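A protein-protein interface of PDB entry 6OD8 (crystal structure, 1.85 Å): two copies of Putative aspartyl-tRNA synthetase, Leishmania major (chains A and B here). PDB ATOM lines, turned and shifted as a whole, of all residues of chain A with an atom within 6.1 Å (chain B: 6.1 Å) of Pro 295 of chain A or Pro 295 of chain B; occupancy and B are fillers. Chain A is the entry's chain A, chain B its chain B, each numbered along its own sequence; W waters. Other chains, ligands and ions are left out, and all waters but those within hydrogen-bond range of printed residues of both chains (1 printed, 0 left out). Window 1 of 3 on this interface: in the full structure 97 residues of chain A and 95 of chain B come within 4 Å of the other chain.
The side-chain carboxylate (OE1) of Glu 310 of chain B sits at hydrogen-bond distance from the backbone NH (N) of Lys 247 of chain A (2.6 Å).
The side-chain carboxylate (OE2) of Glu 310 of chain A sits at hydrogen-bond distance from the backbone NH (N) of Lys 247 of chain B, at 2.7 Å.
The backbone NH of Ala 272 of chain B is in hydrogen-bond range of the backbone carbonyl oxygen of Lys 247 of chain B, 2.7 Å away.
N of Ala 272 of chain A sits at hydrogen-bond distance from O of Lys 247 of chain A.
The backbone carbonyl oxygen (O) of Ser 245 of chain B lies within hydrogen-bond range of the side-chain amino group (NZ) of Lys 247 of chain B (3.1 Å).
Among the printed residues, merely in contact across the chains: Lys 247 of chain A with Pro 295 of chain B, Pro 295 of chain A with Lys 247 of chain B and Pro 295 of chain A with Pro 295 of chain B.
Printed residues of chain B within 4 Å of Lys 247 of chain A: Pro 295 (3.9 Å) and Glu 310 (2.6 Å).
Ala 272 of chain A touches none of the printed residues of chain B.
Of chain B, only Lys 247 (3.8 Å) and Pro 295 (3.4 Å) come within 4 Å of Pro 295 of chain A.
Of the printed residues of chain B, Glu 310 of chain A touches Lys 247 (2.7 Å).
Of the printed residues of chain A, Lys 247 of chain B touches Pro 295 and Glu 310.
Pro 295 of chain B touches just these residues of chain A: Lys 247 and Pro 295.
Val 296 of chain B touches none of the printed residues of chain A.
Of the printed residues of chain A, Glu 310 of chain B touches Lys 247 (2.6 Å).
The nearest residue of chain B that does not touch Pro 295 of chain A is Gly 294 of chain B (5.2 Å).
The nearest residue of chain A that does not touch Pro 295 of chain B is Gly 294 of chain A (5.2 Å).
The nearest printed residue of chain B that does not touch Glu 310 of chain A is Ser 245 of chain B (4.3 Å).
Of the 14 printed residues of chain A, 3 touch a printed residue of chain B.
Hydrophobic or aromatic side chains of chain A that line the printed part of chain B: Pro 295.
Hydrophobic or aromatic side chains of chain B that line the printed part of chain A: Pro 295.
Among the printed residues, no Asp or Glu carboxylate lies within 4 Å of a Lys or Arg side-chain nitrogen of the other chain.
Lys 247 of chain A touches Pro 295 of chain B, and with the chains exchanged Pro 295 of chain A touches Lys 247 of chain B.
Lys 247 of chain A touches Glu 310 of chain B, and with the chains exchanged Glu 310 of chain A touches Lys 247 of chain B.
Pro 295 of chain B touches its own counterpart, Pro 295 of chain A.
Water W1 lies within hydrogen-bond range of O of Val 293 of chain B (2.8 Å) and O of Val 293 of chain A (2.9 Å).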
ATOM      1  N   LYS A 247     -31.539  25.636  23.641  1.00  0.00           N
ATOM      2  CA  LYS A 247     -31.425  24.345  22.991  1.00  0.00           C
ATOM      3  C   LYS A 247     -32.664  24.001  22.186  1.00  0.00           C
ATOM      4  O   LYS A 247     -32.572  23.184  21.259  1.00  0.00           O
ATOM      5  CB  LYS A 247     -31.133  23.253  24.038  1.00  0.00           C
ATOM      6  CG  LYS A 247     -30.035  23.649  25.039  1.00  0.00           C
ATOM      7  CD  LYS A 247     -28.755  24.133  24.332  1.00  0.00           C
ATOM      8  CE  LYS A 247     -27.774  24.877  25.268  1.00  0.00           C
ATOM      9  NZ  LYS A 247     -26.683  25.566  24.432  1.00  0.00           N
ATOM     10  N   ALA A 272     -31.238  21.955  19.167  1.00  0.00           N
ATOM     11  CA  ALA A 272     -30.067  22.510  18.512  1.00  0.00           C
ATOM     12  C   ALA A 272     -28.901  21.534  18.584  1.00  0.00           C
ATOM     13  O   ALA A 272     -28.625  20.933  19.627  1.00  0.00           O
ATOM     14  CB  ALA A 272     -29.678  23.838  19.170  1.00  0.00           C
ATOM     15  N   GLN A 273     -28.209  21.380  17.464  1.00  0.00           N
ATOM     16  CA  GLN A 273     -27.068  20.481  17.446  1.00  0.00           C
ATOM     17  C   GLN A 273     -25.900  21.091  18.180  1.00  0.00           C
ATOM     18  O   GLN A 273     -25.051  20.366  18.714  1.00  0.00           O
ATOM     19  CB  GLN A 273     -26.669  20.155  15.989  1.00  0.00           C
ATOM     20  N   SER A 274     -25.842  22.416  18.219  1.00  0.00           N
ATOM     21  CA  SER A 274     -24.751  23.128  18.860  1.00  0.00           C
ATOM     22  C   SER A 274     -25.170  24.584  18.969  1.00  0.00           C
ATOM     23  O   SER A 274     -26.116  24.997  18.292  1.00  0.00           O
ATOM     24  CB  SER A 274     -23.448  22.996  18.055  1.00  0.00           C
ATOM     25  OG  SER A 274     -23.398  24.009  17.089  1.00  0.00           O
ATOM     26  N   PRO A 275     -24.485  25.376  19.806  1.00  0.00           N
ATOM     27  CA  PRO A 275     -24.843  26.796  19.906  1.00  0.00           C
ATOM     28  C   PRO A 275     -24.211  27.643  18.804  1.00  0.00           C
ATOM     29  O   PRO A 275     -24.135  28.857  18.954  1.00  0.00           O
ATOM     30  CB  PRO A 275     -24.319  27.181  21.289  1.00  0.00           C
ATOM     31  CG  PRO A 275     -23.059  26.351  21.407  1.00  0.00           C
ATOM     32  CD  PRO A 275     -23.397  25.024  20.740  1.00  0.00           C
ATOM     33  N   VAL A 293     -20.886  26.313  27.906  1.00  0.00           N
ATOM     34  CA  VAL A 293     -20.746  24.910  28.281  1.00  0.00           C
ATOM     35  C   VAL A 293     -22.159  24.373  28.415  1.00  0.00           C
ATOM     36  O   VAL A 293     -22.916  24.850  29.261  1.00  0.00           O
ATOM     37  CB  VAL A 293     -19.972  24.728  29.598  1.00  0.00           C
ATOM     38  CG1 VAL A 293     -19.884  23.223  29.973  1.00  0.00           C
ATOM     39  CG2 VAL A 293     -18.594  25.348  29.515  1.00  0.00           C
ATOM     40  N   GLY A 294     -22.546  23.438  27.554  1.00  0.00           N
ATOM     41  CA  GLY A 294     -23.895  22.942  27.631  1.00  0.00           C
ATOM     42  C   GLY A 294     -24.146  21.773  26.712  1.00  0.00           C
ATOM     43  O   GLY A 294     -23.278  21.371  25.928  1.00  0.00           O
ATOM     44  N   PRO A 295     -25.355  21.222  26.782  1.00  0.00           N
ATOM     45  CA  PRO A 295     -25.672  20.037  25.985  1.00  0.00           C
ATOM     46  C   PRO A 295     -25.727  20.345  24.502  1.00  0.00           C
ATOM     47  O   PRO A 295     -26.125  21.431  24.076  1.00  0.00           O
ATOM     48  CB  PRO A 295     -27.053  19.596  26.487  1.00  0.00           C
ATOM     49  CG  PRO A 295     -27.501  20.606  27.491  1.00  0.00           C
ATOM     50  CD  PRO A 295     -26.415  21.591  27.751  1.00  0.00           C
ATOM     51  N   VAL A 296     -25.347  19.338  23.722  1.00  0.00           N
ATOM     52  CA  VAL A 296     -25.442  19.355  22.270  1.00  0.00           C
ATOM     53  C   VAL A 296     -26.039  18.013  21.866  1.00  0.00           C
ATOM     54  O   VAL A 296     -25.984  17.035  22.611  1.00  0.00           O
ATOM     55  CB  VAL A 296     -24.077  19.603  21.607  1.00  0.00           C
ATOM     56  CG1 VAL A 296     -23.598  21.010  21.944  1.00  0.00           C
ATOM     57  CG2 VAL A 296     -23.069  18.618  22.077  1.00  0.00           C
ATOM     58  N   PHE A 297     -26.657  17.981  20.693  1.00  0.00           N
ATOM     59  CA  PHE A 297     -27.456  16.830  20.287  1.00  0.00           C
ATOM     60  C   PHE A 297     -27.097  16.485  18.850  1.00  0.00           C
ATOM     61  O   PHE A 297     -27.019  17.379  18.005  1.00  0.00           O
ATOM     62  CB  PHE A 297     -28.958  17.126  20.450  1.00  0.00           C
ATOM     63  CG  PHE A 297     -29.357  17.521  21.868  1.00  0.00           C
ATOM     64  CD1 PHE A 297     -29.659  16.551  22.817  1.00  0.00           C
ATOM     65  CD2 PHE A 297     -29.421  18.866  22.250  1.00  0.00           C
ATOM     66  CE1 PHE A 297     -30.030  16.907  24.134  1.00  0.00           C
ATOM     67  CE2 PHE A 297     -29.776  19.236  23.561  1.00  0.00           C
ATOM     68  CZ  PHE A 297     -30.081  18.241  24.511  1.00  0.00           C
ATOM     69  N   GLU A 310     -26.468  12.551  22.741  1.00  0.00           N
ATOM     70  CA  GLU A 310     -26.454  13.759  23.533  1.00  0.00           C
ATOM     71  C   GLU A 310     -25.095  13.825  24.186  1.00  0.00           C
ATOM     72  O   GLU A 310     -24.644  12.830  24.768  1.00  0.00           O
ATOM     73  CB  GLU A 310     -27.569  13.747  24.610  1.00  0.00           C
ATOM     74  CG  GLU A 310     -27.394  14.909  25.581  1.00  0.00           C
ATOM     75  CD  GLU A 310     -28.551  15.073  26.582  1.00  0.00           C
ATOM     76  OE1 GLU A 310     -29.515  14.274  26.559  1.00  0.00           O
ATOM     77  OE2 GLU A 310     -28.489  16.024  27.385  1.00  0.00           O
ATOM     78  N   PHE A 311     -24.443  14.979  24.106  1.00  0.00           N
ATOM     79  CA  PHE A 311     -23.216  15.135  24.887  1.00  0.00           C
ATOM     80  C   PHE A 311     -23.084  16.599  25.293  1.00  0.00           C
ATOM     81  O   PHE A 311     -24.077  17.337  25.350  1.00  0.00           O
ATOM     82  CB  PHE A 311     -22.007  14.550  24.126  1.00  0.00           C
ATOM     83  CG  PHE A 311     -21.783  15.132  22.761  1.00  0.00           C
ATOM     84  CD1 PHE A 311     -20.729  16.017  22.540  1.00  0.00           C
ATOM     85  CD2 PHE A 311     -22.590  14.762  21.689  1.00  0.00           C
ATOM     86  CE1 PHE A 311     -20.483  16.537  21.262  1.00  0.00           C
ATOM     87  CE2 PHE A 311     -22.362  15.283  20.411  1.00  0.00           C
ATOM     88  CZ  PHE A 311     -21.305  16.170  20.201  1.00  0.00           C
ATOM     89  N   VAL A 312     -21.875  17.003  25.646  1.00  0.00           N
ATOM     90  CA  VAL A 312     -21.630  18.323  26.214  1.00  0.00           C
ATOM     91  C   VAL A 312     -20.604  19.026  25.348  1.00  0.00           C
ATOM     92  O   VAL A 312     -19.518  18.481  25.092  1.00  0.00           O
ATOM     93  CB  VAL A 312     -21.128  18.261  27.671  1.00  0.00           C
ATOM     94  CG1 VAL A 312     -20.765  19.682  28.143  1.00  0.00           C
ATOM     95  CG2 VAL A 312     -22.172  17.581  28.595  1.00  0.00           C
ATOM     96  N   GLY A 313     -20.954  20.228  24.892  1.00  0.00           N
ATOM     97  CA  GLY A 313     -20.067  21.036  24.076  1.00  0.00           C
ATOM     98  C   GLY A 313     -19.426  22.151  24.884  1.00  0.00           C
ATOM     99  O   GLY A 313     -20.085  22.817  25.684  1.00  0.00           O
ATOM    100  N   SER B 245     -25.588  15.840  33.383  1.00  0.00           N
ATOM    101  CA  SER B 245     -26.566  14.769  33.283  1.00  0.00           C
ATOM    102  C   SER B 245     -27.465  15.003  32.079  1.00  0.00           C
ATOM    103  O   SER B 245     -27.567  16.132  31.582  1.00  0.00           O
ATOM    104  CB  SER B 245     -27.402  14.678  34.576  1.00  0.00           C
ATOM    105  OG  SER B 245     -28.131  15.858  34.839  1.00  0.00           O
ATOM    106  N   LYS B 247     -30.331  15.659  29.305  1.00  0.00           N
ATOM    107  CA  LYS B 247     -31.586  16.385  29.232  1.00  0.00           C
ATOM    108  C   LYS B 247     -32.666  15.583  28.513  1.00  0.00           C
ATOM    109  O   LYS B 247     -33.855  15.870  28.681  1.00  0.00           O
ATOM    110  CB  LYS B 247     -31.368  17.751  28.548  1.00  0.00           C
ATOM    111  CG  LYS B 247     -30.201  18.576  29.135  1.00  0.00           C
ATOM    112  CD  LYS B 247     -30.275  18.746  30.656  1.00  0.00           C
ATOM    113  CE  LYS B 247     -28.878  19.040  31.218  1.00  0.00           C
ATOM    114  NZ  LYS B 247     -28.851  18.771  32.690  1.00  0.00           N
ATOM    115  N   ALA B 272     -35.946  16.765  30.186  1.00  0.00           N
ATOM    116  CA  ALA B 272     -35.930  16.815  31.647  1.00  0.00           C
ATOM    117  C   ALA B 272     -36.310  18.196  32.169  1.00  0.00           C
ATOM    118  O   ALA B 272     -35.834  19.224  31.679  1.00  0.00           O
ATOM    119  CB  ALA B 272     -34.542  16.430  32.169  1.00  0.00           C
ATOM    120  N   GLN B 273     -37.168  18.214  33.203  1.00  0.00           N
ATOM    121  CA  GLN B 273     -37.523  19.472  33.855  1.00  0.00           C
ATOM    122  C   GLN B 273     -36.372  20.018  34.670  1.00  0.00           C
ATOM    123  O   GLN B 273     -36.327  21.217  34.962  1.00  0.00           O
ATOM    124  CB  GLN B 273     -38.708  19.277  34.804  1.00  0.00           C
ATOM    125  CG  GLN B 273     -40.072  19.292  34.151  1.00  0.00           C
ATOM    126  CD  GLN B 273     -41.184  19.417  35.183  1.00  0.00           C
ATOM    127  OE1 GLN B 273     -42.221  20.026  34.923  1.00  0.00           O
ATOM    128  NE2 GLN B 273     -40.961  18.849  36.365  1.00  0.00           N
ATOM    129  N   SER B 274     -35.490  19.138  35.108  1.00  0.00           N
ATOM    130  CA  SER B 274     -34.378  19.510  35.962  1.00  0.00           C
ATOM    131  C   SER B 274     -33.495  18.283  36.112  1.00  0.00           C
ATOM    132  O   SER B 274     -33.935  17.169  35.814  1.00  0.00           O
ATOM    133  CB  SER B 274     -34.872  19.997  37.337  1.00  0.00           C
ATOM    134  OG  SER B 274     -35.082  18.902  38.203  1.00  0.00           O
ATOM    135  N   PRO B 275     -32.256  18.459  36.562  1.00  0.00           N
ATOM    136  CA  PRO B 275     -31.399  17.304  36.846  1.00  0.00           C
ATOM    137  C   PRO B 275     -31.690  16.609  38.167  1.00  0.00           C
ATOM    138  O   PRO B 275     -30.863  15.794  38.581  1.00  0.00           O
ATOM    139  CB  PRO B 275     -29.994  17.918  36.870  1.00  0.00           C
ATOM    140  CG  PRO B 275     -30.217  19.336  37.298  1.00  0.00           C
ATOM    141  CD  PRO B 275     -31.535  19.737  36.682  1.00  0.00           C
ATOM    142  N   VAL B 293     -24.761  23.116  36.060  1.00  0.00           N
ATOM    143  CA  VAL B 293     -25.276  24.322  35.431  1.00  0.00           C
ATOM    144  C   VAL B 293     -25.720  23.905  34.046  1.00  0.00           C
ATOM    145  O   VAL B 293     -24.893  23.459  33.242  1.00  0.00           O
ATOM    146  CB  VAL B 293     -24.208  25.430  35.365  1.00  0.00           C
ATOM    147  CG1 VAL B 293     -24.765  26.690  34.645  1.00  0.00           C
ATOM    148  CG2 VAL B 293     -23.700  25.776  36.786  1.00  0.00           C
ATOM    149  N   GLY B 294     -27.014  23.999  33.765  1.00  0.00           N
ATOM    150  CA  GLY B 294     -27.440  23.621  32.441  1.00  0.00           C
ATOM    151  C   GLY B 294     -28.899  23.929  32.193  1.00  0.00           C
ATOM    152  O   GLY B 294     -29.626  24.378  33.087  1.00  0.00           O
ATOM    153  N   PRO B 295     -29.353  23.694  30.967  1.00  0.00           N
ATOM    154  CA  PRO B 295     -30.744  24.009  30.628  1.00  0.00           C
ATOM    155  C   PRO B 295     -31.742  23.160  31.393  1.00  0.00           C
ATOM    156  O   PRO B 295     -31.510  21.986  31.706  1.00  0.00           O
ATOM    157  CB  PRO B 295     -30.819  23.723  29.123  1.00  0.00           C
ATOM    158  CG  PRO B 295     -29.690  22.864  28.845  1.00  0.00           C
ATOM    159  CD  PRO B 295     -28.596  23.226  29.791  1.00  0.00           C
ATOM    160  N   VAL B 296     -32.890  23.783  31.667  1.00  0.00           N
ATOM    161  CA  VAL B 296     -34.046  23.098  32.228  1.00  0.00           C
ATOM    162  C   VAL B 296     -35.255  23.576  31.440  1.00  0.00           C
ATOM    163  O   VAL B 296     -35.231  24.636  30.815  1.00  0.00           O
ATOM    164  CB  VAL B 296     -34.213  23.362  33.738  1.00  0.00           C
ATOM    165  CG1 VAL B 296     -32.940  22.928  34.463  1.00  0.00           C
ATOM    166  CG2 VAL B 296     -34.500  24.821  33.993  1.00  0.00           C
ATOM    167  N   PHE B 297     -36.307  22.763  31.453  1.00  0.00           N
ATOM    168  CA  PHE B 297     -37.446  22.931  30.552  1.00  0.00           C
ATOM    169  C   PHE B 297     -38.716  22.758  31.365  1.00  0.00           C
ATOM    170  O   PHE B 297     -38.823  21.803  32.140  1.00  0.00           O
ATOM    171  CB  PHE B 297     -37.413  21.907  29.417  1.00  0.00           C
ATOM    172  CG  PHE B 297     -36.151  21.933  28.628  1.00  0.00           C
ATOM    173  CD1 PHE B 297     -35.989  22.837  27.589  1.00  0.00           C
ATOM    174  CD2 PHE B 297     -35.099  21.085  28.955  1.00  0.00           C
ATOM    175  CE1 PHE B 297     -34.817  22.865  26.847  1.00  0.00           C
ATOM    176  CE2 PHE B 297     -33.916  21.116  28.241  1.00  0.00           C
ATOM    177  CZ  PHE B 297     -33.760  22.017  27.176  1.00  0.00           C
ATOM    178  N   GLU B 310     -37.898  27.525  28.658  1.00  0.00           N
ATOM    179  CA  GLU B 310     -36.556  26.976  28.760  1.00  0.00           C
ATOM    180  C   GLU B 310     -35.724  28.005  29.511  1.00  0.00           C
ATOM    181  O   GLU B 310     -35.818  29.203  29.215  1.00  0.00           O
ATOM    182  CB  GLU B 310     -35.955  26.677  27.349  1.00  0.00           C
ATOM    183  CG  GLU B 310     -34.487  26.245  27.425  1.00  0.00           C
ATOM    184  CD  GLU B 310     -33.801  26.044  26.057  1.00  0.00           C
ATOM    185  OE1 GLU B 310     -32.553  25.896  26.060  1.00  0.00           O
ATOM    186  OE2 GLU B 310     -34.496  26.024  25.009  1.00  0.00           O
ATOM    187  N   PHE B 311     -34.930  27.558  30.481  1.00  0.00           N
ATOM    188  CA  PHE B 311     -34.027  28.481  31.160  1.00  0.00           C
ATOM    189  C   PHE B 311     -32.843  27.684  31.684  1.00  0.00           C
ATOM    190  O   PHE B 311     -32.594  26.558  31.251  1.00  0.00           O
ATOM    191  CB  PHE B 311     -34.757  29.300  32.240  1.00  0.00           C
ATOM    192  CG  PHE B 311     -35.492  28.476  33.288  1.00  0.00           C
ATOM    193  CD1 PHE B 311     -34.932  28.266  34.550  1.00  0.00           C
ATOM    194  CD2 PHE B 311     -36.770  27.975  33.027  1.00  0.00           C
ATOM    195  CE1 PHE B 311     -35.633  27.542  35.553  1.00  0.00           C
ATOM    196  CE2 PHE B 311     -37.469  27.256  34.011  1.00  0.00           C
ATOM    197  CZ  PHE B 311     -36.892  27.035  35.271  1.00  0.00           C
ATOM    198  N   VAL B 312     -32.064  28.287  32.569  1.00  0.00           N
ATOM    199  CA  VAL B 312     -30.823  27.683  33.025  1.00  0.00           C
ATOM    200  C   VAL B 312     -30.949  27.398  34.521  1.00  0.00           C
ATOM    201  O   VAL B 312     -31.231  28.310  35.304  1.00  0.00           O
ATOM    202  CB  VAL B 312     -29.613  28.589  32.742  1.00  0.00           C
ATOM    203  CG1 VAL B 312     -28.349  27.978  33.367  1.00  0.00           C
ATOM    204  CG2 VAL B 312     -29.443  28.822  31.179  1.00  0.00           C
ATOM    205  N   GLY B 313     -30.724  26.147  34.910  1.00  0.00           N
ATOM    206  CA  GLY B 313     -30.751  25.756  36.308  1.00  0.00           C
ATOM    207  C   GLY B 313     -29.359  25.717  36.919  1.00  0.00           C
ATOM    208  O   GLY B 313     -28.406  25.204  36.310  1.00  0.00           O
HETATM  209  O   HOH W   1     -22.614  24.602  32.127  1.00  0.00           O
